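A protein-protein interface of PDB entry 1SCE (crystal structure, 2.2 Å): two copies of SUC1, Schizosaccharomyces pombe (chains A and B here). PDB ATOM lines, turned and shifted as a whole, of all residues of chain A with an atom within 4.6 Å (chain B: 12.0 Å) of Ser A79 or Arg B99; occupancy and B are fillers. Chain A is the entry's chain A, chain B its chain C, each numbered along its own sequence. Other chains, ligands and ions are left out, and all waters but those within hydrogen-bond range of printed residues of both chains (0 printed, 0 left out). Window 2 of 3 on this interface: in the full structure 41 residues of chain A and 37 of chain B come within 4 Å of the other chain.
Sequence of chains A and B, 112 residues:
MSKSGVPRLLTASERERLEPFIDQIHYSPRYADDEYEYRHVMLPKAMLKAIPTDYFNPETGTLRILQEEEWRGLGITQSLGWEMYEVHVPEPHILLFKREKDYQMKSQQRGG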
ATOM      1  N   ARG A  30      -1.947 -19.451 -18.562  1.00  0.00           N
ATOM      2  CA  ARG A  30      -1.357 -20.201 -19.665  1.00  0.00           C
ATOM      3  C   ARG A  30      -0.536 -21.335 -19.042  1.00  0.00           C
ATOM      4  O   ARG A  30       0.368 -21.074 -18.237  1.00  0.00           O
ATOM      5  CB  ARG A  30      -0.435 -19.298 -20.495  1.00  0.00           C
ATOM      6  CG  ARG A  30       0.649 -20.034 -21.243  1.00  0.00           C
ATOM      7  CD  ARG A  30       1.387 -19.129 -22.219  1.00  0.00           C
ATOM      8  NE  ARG A  30       2.102 -18.024 -21.582  1.00  0.00           N
ATOM      9  CZ  ARG A  30       3.111 -17.361 -22.149  1.00  0.00           C
ATOM     10  NH1 ARG A  30       3.547 -17.686 -23.370  1.00  0.00           N
ATOM     11  NH2 ARG A  30       3.659 -16.332 -21.519  1.00  0.00           N
ATOM     12  N   GLU A  35       5.862 -29.595 -25.366  1.00  0.00           N
ATOM     13  CA  GLU A  35       5.854 -28.820 -26.604  1.00  0.00           C
ATOM     14  C   GLU A  35       4.620 -28.017 -26.952  1.00  0.00           C
ATOM     15  O   GLU A  35       4.490 -27.547 -28.078  1.00  0.00           O
ATOM     16  CB  GLU A  35       6.232 -29.714 -27.790  1.00  0.00           C
ATOM     17  CG  GLU A  35       5.617 -31.094 -27.768  1.00  0.00           C
ATOM     18  CD  GLU A  35       6.648 -32.170 -28.062  1.00  0.00           C
ATOM     19  OE1 GLU A  35       7.367 -32.586 -27.125  1.00  0.00           O
ATOM     20  OE2 GLU A  35       6.749 -32.591 -29.234  1.00  0.00           O
ATOM     21  N   TYR A  36       3.747 -27.801 -25.979  1.00  0.00           N
ATOM     22  CA  TYR A  36       2.526 -27.048 -26.220  1.00  0.00           C
ATOM     23  C   TYR A  36       2.148 -26.178 -25.037  1.00  0.00           C
ATOM     24  O   TYR A  36       2.525 -26.454 -23.904  1.00  0.00           O
ATOM     25  CB  TYR A  36       1.362 -28.001 -26.512  1.00  0.00           C
ATOM     26  CG  TYR A  36       1.345 -28.574 -27.908  1.00  0.00           C
ATOM     27  CD1 TYR A  36       2.060 -29.721 -28.220  1.00  0.00           C
ATOM     28  CD2 TYR A  36       0.624 -27.953 -28.921  1.00  0.00           C
ATOM     29  CE1 TYR A  36       2.063 -30.233 -29.512  1.00  0.00           C
ATOM     30  CE2 TYR A  36       0.617 -28.452 -30.204  1.00  0.00           C
ATOM     31  CZ  TYR A  36       1.340 -29.589 -30.498  1.00  0.00           C
ATOM     32  OH  TYR A  36       1.365 -30.064 -31.784  1.00  0.00           O
ATOM     33  N   GLU A  37       1.427 -25.107 -25.333  1.00  0.00           N
ATOM     34  CA  GLU A  37       0.910 -24.192 -24.334  1.00  0.00           C
ATOM     35  C   GLU A  37      -0.594 -24.433 -24.393  1.00  0.00           C
ATOM     36  O   GLU A  37      -1.136 -24.656 -25.470  1.00  0.00           O
ATOM     37  CB  GLU A  37       1.260 -22.752 -24.693  1.00  0.00           C
ATOM     38  CG  GLU A  37       2.718 -22.407 -24.371  1.00  0.00           C
ATOM     39  CD  GLU A  37       3.127 -21.005 -24.817  1.00  0.00           C
ATOM     40  OE1 GLU A  37       2.618 -20.523 -25.849  1.00  0.00           O
ATOM     41  OE2 GLU A  37       3.979 -20.391 -24.143  1.00  0.00           O
ATOM     42  N   GLU A  68     -10.372 -18.628 -35.907  1.00  0.00           N
ATOM     43  CA  GLU A  68     -10.005 -17.427 -35.160  1.00  0.00           C
ATOM     44  C   GLU A  68     -11.015 -16.289 -35.304  1.00  0.00           C
ATOM     45  O   GLU A  68     -11.514 -15.757 -34.313  1.00  0.00           O
ATOM     46  CB  GLU A  68      -8.581 -16.974 -35.522  1.00  0.00           C
ATOM     47  CG  GLU A  68      -8.073 -15.785 -34.695  1.00  0.00           C
ATOM     48  CD  GLU A  68      -6.574 -15.847 -34.400  1.00  0.00           C
ATOM     49  OE1 GLU A  68      -5.834 -16.532 -35.138  1.00  0.00           O
ATOM     50  OE2 GLU A  68      -6.131 -15.214 -33.417  1.00  0.00           O
ATOM     51  N   ARG A  72     -13.382 -14.774 -32.348  1.00  0.00           N
ATOM     52  CA  ARG A  72     -13.140 -13.349 -32.096  1.00  0.00           C
ATOM     53  C   ARG A  72     -14.475 -12.634 -32.273  1.00  0.00           C
ATOM     54  O   ARG A  72     -14.736 -11.629 -31.622  1.00  0.00           O
ATOM     55  CB  ARG A  72     -12.055 -12.755 -33.008  1.00  0.00           C
ATOM     56  CG  ARG A  72     -10.638 -13.200 -32.632  1.00  0.00           C
ATOM     57  CD  ARG A  72      -9.553 -12.290 -33.195  1.00  0.00           C
ATOM     58  NE  ARG A  72      -8.197 -12.765 -32.883  1.00  0.00           N
ATOM     59  CZ  ARG A  72      -7.478 -12.386 -31.823  1.00  0.00           C
ATOM     60  NH1 ARG A  72      -7.961 -11.518 -30.941  1.00  0.00           N
ATOM     61  NH2 ARG A  72      -6.265 -12.893 -31.634  1.00  0.00           N
ATOM     62  N   GLN A  78      -7.679 -12.661 -27.261  1.00  0.00           N
ATOM     63  CA  GLN A  78      -6.432 -13.338 -26.922  1.00  0.00           C
ATOM     64  C   GLN A  78      -5.335 -12.916 -27.885  1.00  0.00           C
ATOM     65  O   GLN A  78      -5.572 -12.211 -28.865  1.00  0.00           O
ATOM     66  CB  GLN A  78      -6.575 -14.855 -27.058  1.00  0.00           C
ATOM     67  CG  GLN A  78      -7.411 -15.548 -26.030  1.00  0.00           C
ATOM     68  CD  GLN A  78      -7.558 -17.026 -26.334  1.00  0.00           C
ATOM     69  OE1 GLN A  78      -8.363 -17.424 -27.173  1.00  0.00           O
ATOM     70  NE2 GLN A  78      -6.767 -17.844 -25.663  1.00  0.00           N
ATOM     71  N   SER A  79      -4.143 -13.424 -27.613  1.00  0.00           N
ATOM     72  CA  SER A  79      -2.953 -13.182 -28.409  1.00  0.00           C
ATOM     73  C   SER A  79      -3.094 -13.890 -29.764  1.00  0.00           C
ATOM     74  O   SER A  79      -4.065 -14.620 -30.014  1.00  0.00           O
ATOM     75  CB  SER A  79      -1.751 -13.784 -27.651  1.00  0.00           C
ATOM     76  OG  SER A  79      -0.521 -13.508 -28.289  1.00  0.00           O
ATOM     77  N   LEU A  80      -2.135 -13.666 -30.653  1.00  0.00           N
ATOM     78  CA  LEU A  80      -2.159 -14.369 -31.929  1.00  0.00           C
ATOM     79  C   LEU A  80      -1.567 -15.760 -31.627  1.00  0.00           C
ATOM     80  O   LEU A  80      -0.812 -15.904 -30.670  1.00  0.00           O
ATOM     81  CB  LEU A  80      -1.279 -13.652 -32.965  1.00  0.00           C
ATOM     82  CG  LEU A  80      -1.756 -12.448 -33.785  1.00  0.00           C
ATOM     83  CD1 LEU A  80      -3.166 -12.670 -34.325  1.00  0.00           C
ATOM     84  CD2 LEU A  80      -1.708 -11.214 -32.956  1.00  0.00           C
ATOM     85  N   GLY A  81      -1.962 -16.790 -32.369  1.00  0.00           N
ATOM     86  CA  GLY A  81      -1.362 -18.095 -32.151  1.00  0.00           C
ATOM     87  C   GLY A  81      -2.164 -19.269 -31.640  1.00  0.00           C
ATOM     88  O   GLY A  81      -1.836 -20.410 -31.964  1.00  0.00           O
ATOM     89  N   TRP A  82      -3.199 -19.012 -30.850  1.00  0.00           N
ATOM     90  CA  TRP A  82      -4.013 -20.078 -30.280  1.00  0.00           C
ATOM     91  C   TRP A  82      -4.921 -20.755 -31.284  1.00  0.00           C
ATOM     92  O   TRP A  82      -5.357 -20.151 -32.270  1.00  0.00           O
ATOM     93  CB  TRP A  82      -4.872 -19.543 -29.136  1.00  0.00           C
ATOM     94  CG  TRP A  82      -4.102 -18.925 -28.003  1.00  0.00           C
ATOM     95  CD1 TRP A  82      -3.929 -17.596 -27.767  1.00  0.00           C
ATOM     96  CD2 TRP A  82      -3.427 -19.616 -26.934  1.00  0.00           C
ATOM     97  NE1 TRP A  82      -3.190 -17.411 -26.623  1.00  0.00           N
ATOM     98  CE2 TRP A  82      -2.867 -18.630 -26.091  1.00  0.00           C
ATOM     99  CE3 TRP A  82      -3.239 -20.965 -26.615  1.00  0.00           C
ATOM    100  CZ2 TRP A  82      -2.131 -18.949 -24.951  1.00  0.00           C
ATOM    101  CZ3 TRP A  82      -2.505 -21.281 -25.481  1.00  0.00           C
ATOM    102  CH2 TRP A  82      -1.958 -20.272 -24.660  1.00  0.00           C
ATOM    103  N   GLU A  83      -5.198 -22.024 -31.038  1.00  0.00           N
ATOM    104  CA  GLU A  83      -6.094 -22.770 -31.902  1.00  0.00           C
ATOM    105  C   GLU A  83      -7.000 -23.649 -31.046  1.00  0.00           C
ATOM    106  O   GLU A  83      -6.542 -24.379 -30.164  1.00  0.00           O
ATOM    107  CB  GLU A  83      -5.315 -23.566 -32.956  1.00  0.00           C
ATOM    108  CG  GLU A  83      -4.275 -24.518 -32.419  1.00  0.00           C
ATOM    109  CD  GLU A  83      -3.102 -24.701 -33.373  1.00  0.00           C
ATOM    110  OE1 GLU A  83      -3.266 -24.480 -34.601  1.00  0.00           O
ATOM    111  OE2 GLU A  83      -2.008 -25.064 -32.886  1.00  0.00           O
ATOM    112  N   ASP B  34       5.166 -38.472 -25.595  1.00  0.00           N
ATOM    113  CA  ASP B  34       6.282 -38.166 -24.698  1.00  0.00           C
ATOM    114  C   ASP B  34       6.227 -38.967 -23.394  1.00  0.00           C
ATOM    115  O   ASP B  34       7.232 -39.530 -22.959  1.00  0.00           O
ATOM    116  CB  ASP B  34       6.315 -36.671 -24.364  1.00  0.00           C
ATOM    117  CG  ASP B  34       6.684 -35.812 -25.558  1.00  0.00           C
ATOM    118  OD1 ASP B  34       7.891 -35.709 -25.869  1.00  0.00           O
ATOM    119  OD2 ASP B  34       5.765 -35.232 -26.177  1.00  0.00           O
ATOM    120  N   LEU B  95     -14.135 -23.495 -23.455  1.00  0.00           N
ATOM    121  CA  LEU B  95     -13.537 -23.716 -24.766  1.00  0.00           C
ATOM    122  C   LEU B  95     -12.058 -23.993 -24.532  1.00  0.00           C
ATOM    123  O   LEU B  95     -11.418 -23.331 -23.706  1.00  0.00           O
ATOM    124  CB  LEU B  95     -13.709 -22.482 -25.674  1.00  0.00           C
ATOM    125  CG  LEU B  95     -14.955 -21.579 -25.598  1.00  0.00           C
ATOM    126  CD1 LEU B  95     -15.043 -20.748 -26.862  1.00  0.00           C
ATOM    127  CD2 LEU B  95     -16.225 -22.376 -25.448  1.00  0.00           C
ATOM    128  N   LEU B  96     -11.515 -24.950 -25.274  1.00  0.00           N
ATOM    129  CA  LEU B  96     -10.108 -25.322 -25.142  1.00  0.00           C
ATOM    130  C   LEU B  96      -9.253 -24.778 -26.283  1.00  0.00           C
ATOM    131  O   LEU B  96      -9.648 -24.830 -27.451  1.00  0.00           O
ATOM    132  CB  LEU B  96      -9.962 -26.847 -25.081  1.00  0.00           C
ATOM    133  CG  LEU B  96     -10.757 -27.586 -23.995  1.00  0.00           C
ATOM    134  CD1 LEU B  96     -10.574 -29.118 -24.140  1.00  0.00           C
ATOM    135  CD2 LEU B  96     -10.326 -27.080 -22.609  1.00  0.00           C
ATOM    136  N   PHE B  97      -8.059 -24.311 -25.935  1.00  0.00           N
ATOM    137  CA  PHE B  97      -7.127 -23.753 -26.889  1.00  0.00           C
ATOM    138  C   PHE B  97      -5.720 -24.256 -26.583  1.00  0.00           C
ATOM    139  O   PHE B  97      -5.397 -24.547 -25.425  1.00  0.00           O
ATOM    140  CB  PHE B  97      -7.122 -22.211 -26.797  1.00  0.00           C
ATOM    141  CG  PHE B  97      -8.414 -21.557 -27.197  1.00  0.00           C
ATOM    142  CD1 PHE B  97      -9.413 -21.311 -26.249  1.00  0.00           C
ATOM    143  CD2 PHE B  97      -8.621 -21.146 -28.512  1.00  0.00           C
ATOM    144  CE1 PHE B  97     -10.602 -20.663 -26.610  1.00  0.00           C
ATOM    145  CE2 PHE B  97      -9.799 -20.498 -28.886  1.00  0.00           C
ATOM    146  CZ  PHE B  97     -10.795 -20.254 -27.936  1.00  0.00           C
ATOM    147  N   LYS B  98      -4.883 -24.321 -27.620  1.00  0.00           N
ATOM    148  CA  LYS B  98      -3.488 -24.746 -27.488  1.00  0.00           C
ATOM    149  C   LYS B  98      -2.657 -24.113 -28.609  1.00  0.00           C
ATOM    150  O   LYS B  98      -3.213 -23.575 -29.563  1.00  0.00           O
ATOM    151  CB  LYS B  98      -3.367 -26.270 -27.562  1.00  0.00           C
ATOM    152  CG  LYS B  98      -3.529 -26.831 -28.948  1.00  0.00           C
ATOM    153  CD  LYS B  98      -2.736 -28.097 -29.120  1.00  0.00           C
ATOM    154  CE  LYS B  98      -3.302 -29.212 -28.287  1.00  0.00           C
ATOM    155  NZ  LYS B  98      -4.691 -29.515 -28.710  1.00  0.00           N
ATOM    156  N   ARG B  99      -1.335 -24.157 -28.476  1.00  0.00           N
ATOM    157  CA  ARG B  99      -0.422 -23.606 -29.482  1.00  0.00           C
ATOM    158  C   ARG B  99       1.004 -24.093 -29.180  1.00  0.00           C
ATOM    159  O   ARG B  99       1.331 -24.384 -28.036  1.00  0.00           O
ATOM    160  CB  ARG B  99      -0.496 -22.063 -29.496  1.00  0.00           C
ATOM    161  CG  ARG B  99       0.741 -21.339 -28.968  1.00  0.00           C
ATOM    162  CD  ARG B  99       0.426 -20.321 -27.872  1.00  0.00           C
ATOM    163  NE  ARG B  99       0.233 -18.957 -28.359  1.00  0.00           N
ATOM    164  CZ  ARG B  99       0.706 -17.871 -27.745  1.00  0.00           C
ATOM    165  NH1 ARG B  99       1.407 -17.988 -26.629  1.00  0.00           N
ATOM    166  NH2 ARG B  99       0.443 -16.660 -28.218  1.00  0.00           N
ATOM    167  N   GLU B 100       1.834 -24.216 -30.212  1.00  0.00           N
ATOM    168  CA  GLU B 100       3.209 -24.679 -30.038  1.00  0.00           C
ATOM    169  C   GLU B 100       4.002 -23.699 -29.186  1.00  0.00           C
ATOM    170  O   GLU B 100       3.983 -22.482 -29.435  1.00  0.00           O
ATOM    171  CB  GLU B 100       3.897 -24.855 -31.393  1.00  0.00           C
ATOM    172  CG  GLU B 100       3.095 -25.685 -32.380  1.00  0.00           C
ATOM    173  CD  GLU B 100       3.717 -25.724 -33.767  1.00  0.00           C
ATOM    174  OE1 GLU B 100       4.134 -24.659 -34.283  1.00  0.00           O
ATOM    175  OE2 GLU B 100       3.776 -26.828 -34.348  1.00  0.00           O
ATOM    176  N   LYS B 101       4.697 -24.242 -28.185  1.00  0.00           N
ATOM    177  CA  LYS B 101       5.498 -23.450 -27.266  1.00  0.00           C
ATOM    178  C   LYS B 101       6.771 -22.910 -27.925  1.00  0.00           C
ATOM    179  O   LYS B 101       7.544 -23.674 -28.514  1.00  0.00           O
ATOM    180  CB  LYS B 101       5.863 -24.271 -26.026  1.00  0.00           C
ATOM    181  CG  LYS B 101       6.688 -23.487 -25.027  1.00  0.00           C
ATOM    182  CD  LYS B 101       6.828 -24.199 -23.701  1.00  0.00           C
ATOM    183  CE  LYS B 101       7.892 -25.281 -23.736  1.00  0.00           C
ATOM    184  NZ  LYS B 101       8.019 -25.916 -22.388  1.00  0.00           N
ATOM    185  N   ASP B 102       6.987 -21.602 -27.801  1.00  0.00           N
ATOM    186  CA  ASP B 102       8.152 -20.949 -28.366  1.00  0.00           C
ATOM    187  C   ASP B 102       9.170 -20.498 -27.320  1.00  0.00           C
ATOM    188  O   ASP B 102       8.811 -20.067 -26.221  1.00  0.00           O
ATOM    189  CB  ASP B 102       7.739 -19.734 -29.198  1.00  0.00           C
ATOM    190  CG  ASP B 102       8.888 -19.189 -30.037  1.00  0.00           C
ATOM    191  OD1 ASP B 102       9.367 -19.932 -30.919  1.00  0.00           O
ATOM    192  OD2 ASP B 102       9.326 -18.037 -29.812  1.00  0.00           O
ATOM    193  N   TYR B 103      10.440 -20.570 -27.709  1.00  0.00           N
ATOM    194  CA  TYR B 103      11.587 -20.156 -26.900  1.00  0.00           C
ATOM    195  C   TYR B 103      12.810 -20.222 -27.817  1.00  0.00           C
ATOM    196  O   TYR B 103      12.670 -20.568 -28.996  1.00  0.00           O
ATOM    197  CB  TYR B 103      11.769 -21.074 -25.674  1.00  0.00           C
ATOM    198  CG  TYR B 103      11.942 -22.551 -25.973  1.00  0.00           C
ATOM    199  CD1 TYR B 103      10.857 -23.338 -26.354  1.00  0.00           C
ATOM    200  CD2 TYR B 103      13.191 -23.167 -25.853  1.00  0.00           C
ATOM    201  CE1 TYR B 103      11.008 -24.700 -26.610  1.00  0.00           C
ATOM    202  CE2 TYR B 103      13.352 -24.535 -26.103  1.00  0.00           C
ATOM    203  CZ  TYR B 103      12.255 -25.290 -26.487  1.00  0.00           C
ATOM    204  OH  TYR B 103      12.411 -26.625 -26.795  1.00  0.00           O
ATOM    205  N   MET B 105      14.748 -22.108 -29.064  1.00  0.00           N
ATOM    206  CA  MET B 105      14.786 -23.559 -29.309  1.00  0.00           C
ATOM    207  C   MET B 105      15.226 -24.032 -30.691  1.00  0.00           C
ATOM    208  O   MET B 105      14.944 -25.171 -31.088  1.00  0.00           O
ATOM    209  CB  MET B 105      13.380 -24.109 -29.120  1.00  0.00           C
ATOM    210  CG  MET B 105      12.339 -23.449 -29.996  1.00  0.00           C
ATOM    211  SD  MET B 105      10.838 -24.409 -30.066  1.00  0.00           S
ATOM    212  CE  MET B 105      11.435 -25.881 -30.867  1.00  0.00           C
ATOM    213  N   LYS B 106      15.844 -23.160 -31.464  1.00  0.00           N
ATOM    214  CA  LYS B 106      16.266 -23.558 -32.788  1.00  0.00           C
ATOM    215  C   LYS B 106      17.781 -23.339 -32.823  1.00  0.00           C
ATOM    216  O   LYS B 106      18.281 -22.416 -33.469  1.00  0.00           O
ATOM    217  CB  LYS B 106      15.489 -22.730 -33.824  1.00  0.00           C
ATOM    218  CG  LYS B 106      14.314 -21.932 -33.190  1.00  0.00           C
ATOM    219  CD  LYS B 106      12.923 -22.256 -33.750  1.00  0.00           C
ATOM    220  CE  LYS B 106      12.603 -23.750 -33.687  1.00  0.00           C
ATOM    221  NZ  LYS B 106      11.201 -24.053 -34.082  1.00  0.00           N
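O of Glu A35 is in hydrogen-bond range of N of Lys B101 (3.3 Å).
NH1 of Arg B99 lies within salt-bridge range of OE1 of Glu A37.
NH2 of Arg B99 lies within hydrogen-bond range of OG of Ser A79 (3.3 Å).
NH2 of Arg B99 is in hydrogen-bond range of O of Leu A80 (2.9 Å).
The backbone NH of Glu A83 lies within hydrogen-bond range of the backbone carbonyl oxygen of Lys B98 (2.9 Å).
The side-chain carboxylate of Asp B34 sits close to the side-chain carboxylate of Glu A35 (3.2 Å).
OE2 of Glu A37 lies within salt-bridge range of NH1 of Arg A30 (2.8 Å).
The backbone carbonyl oxygen (O) of Gln A78 lies within hydrogen-bond range of the guanidinium group (NH2) of Arg A72 (2.9 Å).
The guanidinium group (NH2) of Arg A72 lies within hydrogen-bond range of the backbone carbonyl oxygen (O) of Ser A79, at 3.2 Å.
Among the printed residues, pairs that only touch across the chains: Glu A37 with Lys B98 (3.1 Å), Gly A81 with Arg B99 (3.3 Å), Tyr A36 with Lys B98 (3.4 Å), Glu A83 with Phe B97 (3.4 Å), Tyr A36 with Arg B99 (3.4 Å), Trp A82 with Lys B98 (3.7 Å), Glu A35 with Glu B100 (3.7 Å), Gln A78 with Phe B97 (3.8 Å), Trp A82 with Arg B99 (3.9 Å) and Arg A30 with Arg B99 (3.9 Å).
Of chain B, only Arg B99 comes within 4 Å of Ser A79.
Arg B99 touches just these residues of chain A: Arg A30 (3.9 Å), Tyr A36 (3.4 Å), Glu A37 (2.8 Å), Ser A79 (3.3 Å), Leu A80 (2.9 Å), Gly A81 (3.3 Å) and Trp A82 (3.9 Å).
Gln A78 touches one residue of chain B.
Leu A80 touches just one residue of chain B: Arg B99.
Gly A81 touches just one residue of chain B: Arg B99 (3.3 Å).
Printed residues of chain B within 4 Å of Glu A83: Phe B97 and Lys B98.
Of the printed residues of chain B, Glu A35 touches Asp B34 (3.2 Å), Glu B100 (3.7 Å) and Lys B101 (3.3 Å).
Of the printed residues of chain A, Lys B98 touches Tyr A36, Glu A37, Trp A82 and Glu A83.
The nearest residue of chain B that does not touch Ser A79 is Phe B97 (8.1 Å).
The nearest residue of chain A that does not touch Arg B99 is Glu A83 (4.03 Å).
The nearest printed residue of chain A that does not touch Phe B97 is Trp A82 (4.1 Å).
Of the 12 printed residues of chain B, 6 touch a printed residue of chain A.
Printed residues of chain B that touch a printed residue of chain A: Asp B34, Phe B97, Lys B98, Arg B99, Glu B100 and Lys B101.
Along chain B the printed residues that touch a printed residue of chain A span positions 34 to 101.
Among the printed residues, 16 pairs touch across the chains.
Among the printed residues, Asp or Glu carboxylates within 4 Å of a Lys or Arg side-chain nitrogen of the other chain: Glu A37 with Arg B99 (2.9 Å).
No position is printed for both chains.
Of the 16 pairs that touch across the chains among the printed residues, none has its exchanged pair printed and touching as well.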
